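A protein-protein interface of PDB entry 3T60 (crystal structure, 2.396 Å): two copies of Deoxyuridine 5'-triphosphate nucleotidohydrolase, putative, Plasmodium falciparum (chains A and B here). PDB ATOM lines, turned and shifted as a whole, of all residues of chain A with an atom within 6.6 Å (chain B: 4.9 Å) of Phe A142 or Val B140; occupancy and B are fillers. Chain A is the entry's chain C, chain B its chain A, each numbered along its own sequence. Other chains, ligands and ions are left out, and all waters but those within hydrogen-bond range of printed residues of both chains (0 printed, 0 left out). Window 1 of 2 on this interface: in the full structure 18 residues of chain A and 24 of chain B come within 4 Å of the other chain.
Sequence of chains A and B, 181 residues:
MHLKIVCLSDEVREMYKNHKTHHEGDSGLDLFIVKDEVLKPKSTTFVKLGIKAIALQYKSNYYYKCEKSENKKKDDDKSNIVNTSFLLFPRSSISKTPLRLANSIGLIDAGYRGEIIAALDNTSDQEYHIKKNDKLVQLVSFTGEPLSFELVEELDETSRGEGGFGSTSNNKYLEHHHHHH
The side-chain hydroxyl (OG) of Ser B27 sits at hydrogen-bond distance from the side-chain hydroxyl (OG) of Ser A85 (3.0 Å).
The backbone carbonyl oxygen (O) of Leu B87 is in hydrogen-bond range of the backbone NH (N) of Val B140, at 2.8 Å.
N of Phe B89 sits at hydrogen-bond distance from O of Gln B138.
The side-chain hydroxyl (OG) of Ser B141 is in hydrogen-bond range of the backbone NH (N) of Thr B143 (2.9 Å).
The backbone carbonyl oxygen (O) of Leu A87 is in hydrogen-bond range of the backbone NH (N) of Val A140.
Phe A142 touches Ser B141, but with the chains exchanged Ser A141 does not touch Phe B142 (7.0 Å).
Phe B142 touches its own counterpart, Phe A142.
Phe A142 touches Thr B143, but with the chains exchanged Thr A143 does not touch Phe B142 (5.5 Å).
Phe A142 touches Gly B144, but with the chains exchanged Gly A144 does not touch Phe B142 (7.4 Å).
Positions printed for both chains: 1, 86, 87, 140, 141, 142, 143 and 144.
Of the 10 pairs that touch across the chains among the printed residues, 1 has its exchanged pair printed and touching as well.
Ser A85 touches Gly B144.
CD2 of Leu A87 touches CZ of Phe B89, at 3.97 Å.
Leu A107 touches Ser B27 (CD1 to OG, 3.6 Å).
Leu A107 touches Gln B138 (CD2 to OE1, 3.9 Å).
CG2 of Val B140 touches CE1 of Phe A142, at 3.9 Å.
O of Ser B141 touches CE1 of Phe A142, 3.5 Å away.
Phe B142 touches Phe A142 (O to CD1, 3.5 Å).
Phe A142 touches Thr B143.
Gly B144 touches Phe A142 (N to CD1, 3.4 Å).
Of the printed residues of chain B, Phe A142 touches Val B140, Ser B141, Phe B142, Thr B143 and Gly B144.
Of chain A, only Phe A142 (3.9 Å) comes within 4 Å of Val B140.
Of the printed residues of chain A, Phe B142 touches Phe A142.
Of the printed residues of chain B, Ser A85 touches Ser B27 and Gly B144.
Of the printed residues of chain B, Leu A87 touches Phe B89 (3.97 Å).
The nearest printed residue of chain B that does not touch Phe A142 is Phe B89 (4.9 Å).
The nearest residue of chain A that does not touch Val B140 is Leu A107 (4.3 Å).
Of the 14 printed residues of chain A, 4 touch a printed residue of chain B.
Printed residues of chain A that touch a printed residue of chain B: Ser A85, Leu A87, Leu A107 and Phe A142.
Hydrophobic or aromatic side chains of chain A that line the printed part of chain B: Leu A87, Leu A107 and Phe A142.
Printed residues of chain B that touch a printed residue of chain A: Ser B27, Phe B89, Gln B138, Val B140, Ser B141, Phe B142, Thr B143 and Gly B144.
Hydrophobic or aromatic side chains of chain B that line the printed part of chain A: Phe B89 and Val B140.
Among the printed residues, 10 pairs touch across the chains.
Among the printed residues, no Asp or Glu carboxylate lies within 4 Å of a Lys or Arg side-chain nitrogen of the other chain.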
ATOM      1  N   MET A   1     -14.438 -10.762  14.929  1.00  0.00           N
ATOM      2  CA  MET A   1     -14.216 -11.882  13.953  1.00  0.00           C
ATOM      3  C   MET A   1     -15.054 -11.543  12.734  1.00  0.00           C
ATOM      4  O   MET A   1     -16.087 -10.923  12.865  1.00  0.00           O
ATOM      5  CB  MET A   1     -14.691 -13.181  14.592  1.00  0.00           C
ATOM      6  CG  MET A   1     -14.666 -14.420  13.723  1.00  0.00           C
ATOM      7  SD  MET A   1     -15.205 -15.871  14.718  1.00  0.00           S
ATOM      8  CE  MET A   1     -16.970 -15.788  14.409  1.00  0.00           C
ATOM      9  N   GLN A  57     -10.113 -14.619  11.560  1.00  0.00           N
ATOM     10  CA  GLN A  57      -9.543 -13.821  12.688  1.00  0.00           C
ATOM     11  C   GLN A  57      -8.073 -13.497  12.434  1.00  0.00           C
ATOM     12  O   GLN A  57      -7.449 -14.132  11.571  1.00  0.00           O
ATOM     13  CB  GLN A  57      -9.654 -14.565  14.017  1.00  0.00           C
ATOM     14  CG  GLN A  57     -10.819 -14.110  14.937  1.00  0.00           C
ATOM     15  CD  GLN A  57     -11.110 -15.097  16.119  1.00  0.00           C
ATOM     16  OE1 GLN A  57     -12.272 -15.375  16.438  1.00  0.00           O
ATOM     17  NE2 GLN A  57     -10.051 -15.598  16.771  1.00  0.00           N
ATOM     18  N   THR A  84     -10.760 -19.759  11.316  1.00  0.00           N
ATOM     19  CA  THR A  84     -10.767 -20.057  12.710  1.00  0.00           C
ATOM     20  C   THR A  84     -11.996 -20.917  13.018  1.00  0.00           C
ATOM     21  O   THR A  84     -12.943 -20.999  12.216  1.00  0.00           O
ATOM     22  CB  THR A  84     -10.643 -18.741  13.539  1.00  0.00           C
ATOM     23  OG1 THR A  84     -10.215 -19.027  14.876  1.00  0.00           O
ATOM     24  CG2 THR A  84     -11.936 -18.026  13.586  1.00  0.00           C
ATOM     25  N   SER A  85     -11.946 -21.633  14.131  1.00  0.00           N
ATOM     26  CA  SER A  85     -13.130 -22.276  14.653  1.00  0.00           C
ATOM     27  C   SER A  85     -14.100 -21.252  15.215  1.00  0.00           C
ATOM     28  O   SER A  85     -13.693 -20.186  15.647  1.00  0.00           O
ATOM     29  CB  SER A  85     -12.704 -23.138  15.799  1.00  0.00           C
ATOM     30  OG  SER A  85     -12.053 -24.218  15.255  1.00  0.00           O
ATOM     31  N   PHE A  86     -15.379 -21.586  15.258  1.00  0.00           N
ATOM     32  CA  PHE A  86     -16.308 -20.757  16.017  1.00  0.00           C
ATOM     33  C   PHE A  86     -17.455 -21.569  16.656  1.00  0.00           C
ATOM     34  O   PHE A  86     -17.489 -22.795  16.566  1.00  0.00           O
ATOM     35  CB  PHE A  86     -16.806 -19.598  15.124  1.00  0.00           C
ATOM     36  CG  PHE A  86     -17.477 -20.054  13.879  1.00  0.00           C
ATOM     37  CD1 PHE A  86     -16.727 -20.446  12.778  1.00  0.00           C
ATOM     38  CD2 PHE A  86     -18.885 -20.122  13.818  1.00  0.00           C
ATOM     39  CE1 PHE A  86     -17.337 -20.855  11.619  1.00  0.00           C
ATOM     40  CE2 PHE A  86     -19.508 -20.545  12.654  1.00  0.00           C
ATOM     41  CZ  PHE A  86     -18.735 -20.890  11.535  1.00  0.00           C
ATOM     42  N   LEU A  87     -18.393 -20.878  17.284  1.00  0.00           N
ATOM     43  CA  LEU A  87     -19.388 -21.469  18.175  1.00  0.00           C
ATOM     44  C   LEU A  87     -20.800 -21.171  17.778  1.00  0.00           C
ATOM     45  O   LEU A  87     -21.098 -20.128  17.252  1.00  0.00           O
ATOM     46  CB  LEU A  87     -19.174 -20.877  19.539  1.00  0.00           C
ATOM     47  CG  LEU A  87     -17.822 -21.304  20.060  1.00  0.00           C
ATOM     48  CD1 LEU A  87     -17.403 -20.455  21.244  1.00  0.00           C
ATOM     49  CD2 LEU A  87     -17.875 -22.826  20.362  1.00  0.00           C
ATOM     50  N   LEU A 107     -19.759 -26.628  18.203  1.00  0.00           N
ATOM     51  CA  LEU A 107     -18.385 -26.303  17.852  1.00  0.00           C
ATOM     52  C   LEU A 107     -18.191 -26.489  16.307  1.00  0.00           C
ATOM     53  O   LEU A 107     -18.372 -27.561  15.745  1.00  0.00           O
ATOM     54  CB  LEU A 107     -17.413 -27.153  18.703  1.00  0.00           C
ATOM     55  CG  LEU A 107     -15.951 -27.079  18.316  1.00  0.00           C
ATOM     56  CD1 LEU A 107     -15.280 -25.708  18.550  1.00  0.00           C
ATOM     57  CD2 LEU A 107     -15.165 -28.234  18.954  1.00  0.00           C
ATOM     58  N   ILE A 108     -17.903 -25.388  15.600  1.00  0.00           N
ATOM     59  CA  ILE A 108     -17.630 -25.476  14.167  1.00  0.00           C
ATOM     60  C   ILE A 108     -16.123 -25.297  13.901  1.00  0.00           C
ATOM     61  O   ILE A 108     -15.529 -24.204  14.148  1.00  0.00           O
ATOM     62  CB  ILE A 108     -18.521 -24.491  13.409  1.00  0.00           C
ATOM     63  CG1 ILE A 108     -19.967 -24.842  13.729  1.00  0.00           C
ATOM     64  CG2 ILE A 108     -18.299 -24.595  11.911  1.00  0.00           C
ATOM     65  CD1 ILE A 108     -20.830 -23.763  13.743  1.00  0.00           C
ATOM     66  N   VAL A 140     -20.990 -17.274  17.394  1.00  0.00           N
ATOM     67  CA  VAL A 140     -20.129 -16.516  18.309  1.00  0.00           C
ATOM     68  C   VAL A 140     -18.657 -16.882  18.202  1.00  0.00           C
ATOM     69  O   VAL A 140     -18.313 -18.039  17.884  1.00  0.00           O
ATOM     70  CB  VAL A 140     -20.725 -16.316  19.772  1.00  0.00           C
ATOM     71  CG1 VAL A 140     -22.071 -16.934  19.997  1.00  0.00           C
ATOM     72  CG2 VAL A 140     -19.767 -16.371  20.950  1.00  0.00           C
ATOM     73  N   SER A 141     -17.801 -15.880  18.367  1.00  0.00           N
ATOM     74  CA  SER A 141     -16.389 -16.058  18.351  1.00  0.00           C
ATOM     75  C   SER A 141     -15.940 -16.649  19.689  1.00  0.00           C
ATOM     76  O   SER A 141     -16.521 -16.304  20.752  1.00  0.00           O
ATOM     77  CB  SER A 141     -15.710 -14.703  18.104  1.00  0.00           C
ATOM     78  OG  SER A 141     -14.286 -14.794  18.170  1.00  0.00           O
ATOM     79  N   PHE A 142     -14.897 -17.497  19.661  1.00  0.00           N
ATOM     80  CA  PHE A 142     -14.254 -17.965  20.920  1.00  0.00           C
ATOM     81  C   PHE A 142     -13.762 -16.806  21.780  1.00  0.00           C
ATOM     82  O   PHE A 142     -13.722 -16.921  22.990  1.00  0.00           O
ATOM     83  CB  PHE A 142     -13.089 -18.975  20.696  1.00  0.00           C
ATOM     84  CG  PHE A 142     -13.513 -20.435  20.551  1.00  0.00           C
ATOM     85  CD1 PHE A 142     -13.592 -21.274  21.668  1.00  0.00           C
ATOM     86  CD2 PHE A 142     -13.834 -20.957  19.305  1.00  0.00           C
ATOM     87  CE1 PHE A 142     -13.931 -22.662  21.523  1.00  0.00           C
ATOM     88  CE2 PHE A 142     -14.186 -22.317  19.150  1.00  0.00           C
ATOM     89  CZ  PHE A 142     -14.238 -23.156  20.264  1.00  0.00           C
ATOM     90  N   THR A 143     -13.403 -15.679  21.201  1.00  0.00           N
ATOM     91  CA  THR A 143     -12.937 -14.542  22.049  1.00  0.00           C
ATOM     92  C   THR A 143     -14.098 -13.609  22.524  1.00  0.00           C
ATOM     93  O   THR A 143     -13.886 -12.684  23.281  1.00  0.00           O
ATOM     94  CB  THR A 143     -11.937 -13.699  21.268  1.00  0.00           C
ATOM     95  OG1 THR A 143     -12.653 -13.018  20.258  1.00  0.00           O
ATOM     96  CG2 THR A 143     -10.919 -14.550  20.543  1.00  0.00           C
ATOM     97  N   GLY A 144     -15.312 -13.838  22.022  1.00  0.00           N
ATOM     98  CA  GLY A 144     -16.503 -13.072  22.382  1.00  0.00           C
ATOM     99  C   GLY A 144     -16.510 -11.676  21.813  1.00  0.00           C
ATOM    100  O   GLY A 144     -17.324 -10.841  22.228  1.00  0.00           O
ATOM    101  N   GLU A 145     -15.602 -11.442  20.871  1.00  0.00           N
ATOM    102  CA  GLU A 145     -15.433 -10.167  20.181  1.00  0.00           C
ATOM    103  C   GLU A 145     -16.576  -9.929  19.159  1.00  0.00           C
ATOM    104  O   GLU A 145     -17.286 -10.893  18.745  1.00  0.00           O
ATOM    105  CB  GLU A 145     -14.030 -10.082  19.512  1.00  0.00           C
ATOM    106  CG  GLU A 145     -13.954 -10.827  18.170  1.00  0.00           C
ATOM    107  CD  GLU A 145     -12.533 -11.205  17.671  1.00  0.00           C
ATOM    108  OE1 GLU A 145     -12.309 -11.239  16.401  1.00  0.00           O
ATOM    109  OE2 GLU A 145     -11.642 -11.484  18.518  1.00  0.00           O
ATOM    110  N   MET B   1      -3.205 -25.417  21.825  1.00  0.00           N
ATOM    111  CA  MET B   1      -3.098 -25.718  23.294  1.00  0.00           C
ATOM    112  C   MET B   1      -2.645 -27.151  23.407  1.00  0.00           C
ATOM    113  O   MET B   1      -3.059 -27.979  22.597  1.00  0.00           O
ATOM    114  CB  MET B   1      -4.421 -25.496  24.043  1.00  0.00           C
ATOM    115  CG  MET B   1      -4.718 -26.549  25.196  1.00  0.00           C
ATOM    116  SD  MET B   1      -6.385 -26.384  25.919  1.00  0.00           S
ATOM    117  CE  MET B   1      -6.925 -28.100  25.997  1.00  0.00           C
ATOM    118  N   SER B  27      -9.827 -28.379  16.656  1.00  0.00           N
ATOM    119  CA  SER B  27     -10.093 -27.673  17.894  1.00  0.00           C
ATOM    120  C   SER B  27     -10.860 -28.445  19.003  1.00  0.00           C
ATOM    121  O   SER B  27     -10.965 -27.937  20.099  1.00  0.00           O
ATOM    122  CB  SER B  27     -10.634 -26.276  17.588  1.00  0.00           C
ATOM    123  OG  SER B  27     -11.988 -26.363  17.309  1.00  0.00           O
ATOM    124  N   GLY B  28     -11.252 -29.703  18.753  1.00  0.00           N
ATOM    125  CA  GLY B  28     -11.742 -30.622  19.754  1.00  0.00           C
ATOM    126  C   GLY B  28     -11.052 -31.988  19.747  1.00  0.00           C
ATOM    127  O   GLY B  28     -10.858 -32.587  18.686  1.00  0.00           O
ATOM    128  N   PHE B  86      -9.774 -25.498  30.912  1.00  0.00           N
ATOM    129  CA  PHE B  86     -10.324 -25.933  29.640  1.00  0.00           C
ATOM    130  C   PHE B  86     -11.746 -26.465  29.682  1.00  0.00           C
ATOM    131  O   PHE B  86     -12.358 -26.617  30.768  1.00  0.00           O
ATOM    132  CB  PHE B  86      -9.352 -26.913  28.958  1.00  0.00           C
ATOM    133  CG  PHE B  86      -9.056 -28.162  29.747  1.00  0.00           C
ATOM    134  CD1 PHE B  86      -8.113 -28.145  30.775  1.00  0.00           C
ATOM    135  CD2 PHE B  86      -9.663 -29.358  29.412  1.00  0.00           C
ATOM    136  CE1 PHE B  86      -7.797 -29.265  31.487  1.00  0.00           C
ATOM    137  CE2 PHE B  86      -9.353 -30.510  30.113  1.00  0.00           C
ATOM    138  CZ  PHE B  86      -8.386 -30.461  31.136  1.00  0.00           C
ATOM    139  N   LEU B  87     -12.239 -26.802  28.474  1.00  0.00           N
ATOM    140  CA  LEU B  87     -13.662 -27.106  28.247  1.00  0.00           C
ATOM    141  C   LEU B  87     -13.974 -28.553  27.884  1.00  0.00           C
ATOM    142  O   LEU B  87     -13.288 -29.177  27.110  1.00  0.00           O
ATOM    143  CB  LEU B  87     -14.270 -26.139  27.238  1.00  0.00           C
ATOM    144  CG  LEU B  87     -14.189 -24.659  27.624  1.00  0.00           C
ATOM    145  CD1 LEU B  87     -14.526 -23.818  26.400  1.00  0.00           C
ATOM    146  CD2 LEU B  87     -15.123 -24.304  28.868  1.00  0.00           C
ATOM    147  N   PHE B  89     -16.857 -30.438  26.002  1.00  0.00           N
ATOM    148  CA  PHE B  89     -18.020 -30.236  25.114  1.00  0.00           C
ATOM    149  C   PHE B  89     -18.635 -31.615  24.821  1.00  0.00           C
ATOM    150  O   PHE B  89     -17.922 -32.542  24.653  1.00  0.00           O
ATOM    151  CB  PHE B  89     -17.584 -29.712  23.779  1.00  0.00           C
ATOM    152  CG  PHE B  89     -17.567 -28.236  23.651  1.00  0.00           C
ATOM    153  CD1 PHE B  89     -16.673 -27.480  24.354  1.00  0.00           C
ATOM    154  CD2 PHE B  89     -18.425 -27.585  22.739  1.00  0.00           C
ATOM    155  CE1 PHE B  89     -16.641 -26.101  24.201  1.00  0.00           C
ATOM    156  CE2 PHE B  89     -18.370 -26.211  22.566  1.00  0.00           C
ATOM    157  CZ  PHE B  89     -17.506 -25.459  23.310  1.00  0.00           C
ATOM    158  N   GLN B 138     -15.821 -34.236  24.118  1.00  0.00           N
ATOM    159  CA  GLN B 138     -14.501 -33.862  23.643  1.00  0.00           C
ATOM    160  C   GLN B 138     -13.970 -32.638  24.425  1.00  0.00           C
ATOM    161  O   GLN B 138     -14.732 -31.770  24.904  1.00  0.00           O
ATOM    162  CB  GLN B 138     -14.594 -33.519  22.168  1.00  0.00           C
ATOM    163  CG  GLN B 138     -15.357 -32.173  21.949  1.00  0.00           C
ATOM    164  CD  GLN B 138     -15.784 -31.895  20.512  1.00  0.00           C
ATOM    165  OE1 GLN B 138     -15.000 -32.038  19.607  1.00  0.00           O
ATOM    166  NE2 GLN B 138     -17.033 -31.465  20.317  1.00  0.00           N
ATOM    167  N   LEU B 139     -12.644 -32.513  24.436  1.00  0.00           N
ATOM    168  CA  LEU B 139     -11.959 -31.495  25.208  1.00  0.00           C
ATOM    169  C   LEU B 139     -11.661 -30.351  24.273  1.00  0.00           C
ATOM    170  O   LEU B 139     -11.352 -30.592  23.131  1.00  0.00           O
ATOM    171  CB  LEU B 139     -10.689 -32.108  25.786  1.00  0.00           C
ATOM    172  CG  LEU B 139     -10.663 -32.467  27.258  1.00  0.00           C
ATOM    173  CD1 LEU B 139     -11.960 -32.890  27.846  1.00  0.00           C
ATOM    174  CD2 LEU B 139      -9.555 -33.431  27.540  1.00  0.00           C
ATOM    175  N   VAL B 140     -11.857 -29.123  24.694  1.00  0.00           N
ATOM    176  CA  VAL B 140     -11.661 -27.972  23.848  1.00  0.00           C
ATOM    177  C   VAL B 140     -10.999 -26.798  24.567  1.00  0.00           C
ATOM    178  O   VAL B 140     -11.106 -26.674  25.731  1.00  0.00           O
ATOM    179  CB  VAL B 140     -12.863 -27.681  22.865  1.00  0.00           C
ATOM    180  CG1 VAL B 140     -14.009 -28.498  23.116  1.00  0.00           C
ATOM    181  CG2 VAL B 140     -13.217 -26.297  22.735  1.00  0.00           C
ATOM    182  N   SER B 141     -10.255 -25.983  23.855  1.00  0.00           N
ATOM    183  CA  SER B 141      -9.545 -24.870  24.418  1.00  0.00           C
ATOM    184  C   SER B 141     -10.483 -23.677  24.542  1.00  0.00           C
ATOM    185  O   SER B 141     -11.300 -23.440  23.640  1.00  0.00           O
ATOM    186  CB  SER B 141      -8.406 -24.491  23.471  1.00  0.00           C
ATOM    187  OG  SER B 141      -7.842 -23.226  23.874  1.00  0.00           O
ATOM    188  N   PHE B 142     -10.319 -22.873  25.562  1.00  0.00           N
ATOM    189  CA  PHE B 142     -10.991 -21.612  25.619  1.00  0.00           C
ATOM    190  C   PHE B 142     -10.747 -20.735  24.409  1.00  0.00           C
ATOM    191  O   PHE B 142     -11.512 -19.872  24.147  1.00  0.00           O
ATOM    192  CB  PHE B 142     -10.635 -20.881  26.886  1.00  0.00           C
ATOM    193  CG  PHE B 142     -11.593 -21.076  27.989  1.00  0.00           C
ATOM    194  CD1 PHE B 142     -12.774 -20.421  28.010  1.00  0.00           C
ATOM    195  CD2 PHE B 142     -11.309 -21.904  29.013  1.00  0.00           C
ATOM    196  CE1 PHE B 142     -13.620 -20.601  29.002  1.00  0.00           C
ATOM    197  CE2 PHE B 142     -12.174 -22.067  29.995  1.00  0.00           C
ATOM    198  CZ  PHE B 142     -13.324 -21.422  29.986  1.00  0.00           C
ATOM    199  N   THR B 143      -9.696 -20.974  23.655  1.00  0.00           N
ATOM    200  CA  THR B 143      -9.401 -20.176  22.485  1.00  0.00           C
ATOM    201  C   THR B 143      -9.868 -20.793  21.190  1.00  0.00           C
ATOM    202  O   THR B 143      -9.819 -20.167  20.172  1.00  0.00           O
ATOM    203  CB  THR B 143      -7.878 -19.851  22.344  1.00  0.00           C
ATOM    204  OG1 THR B 143      -7.132 -21.024  22.049  1.00  0.00           O
ATOM    205  CG2 THR B 143      -7.324 -19.218  23.557  1.00  0.00           C
ATOM    206  N   GLY B 144     -10.283 -22.041  21.239  1.00  0.00           N
ATOM    207  CA  GLY B 144     -10.670 -22.765  20.062  1.00  0.00           C
ATOM    208  C   GLY B 144      -9.542 -23.171  19.165  1.00  0.00           C
ATOM    209  O   GLY B 144      -9.769 -23.664  18.106  1.00  0.00           O
ATOM    210  N   LEU B 147      -5.597 -28.543  19.053  1.00  0.00           N
ATOM    211  CA  LEU B 147      -5.168 -29.240  20.255  1.00  0.00           C
ATOM    212  C   LEU B 147      -4.123 -30.278  19.916  1.00  0.00           C
ATOM    213  O   LEU B 147      -4.328 -31.075  18.982  1.00  0.00           O
ATOM    214  CB  LEU B 147      -6.345 -29.992  20.956  1.00  0.00           C
ATOM    215  CG  LEU B 147      -7.515 -29.213  21.535  1.00  0.00           C
ATOM    216  CD1 LEU B 147      -8.275 -30.068  22.459  1.00  0.00           C
ATOM    217  CD2 LEU B 147      -7.001 -28.068  22.289  1.00  0.00           C
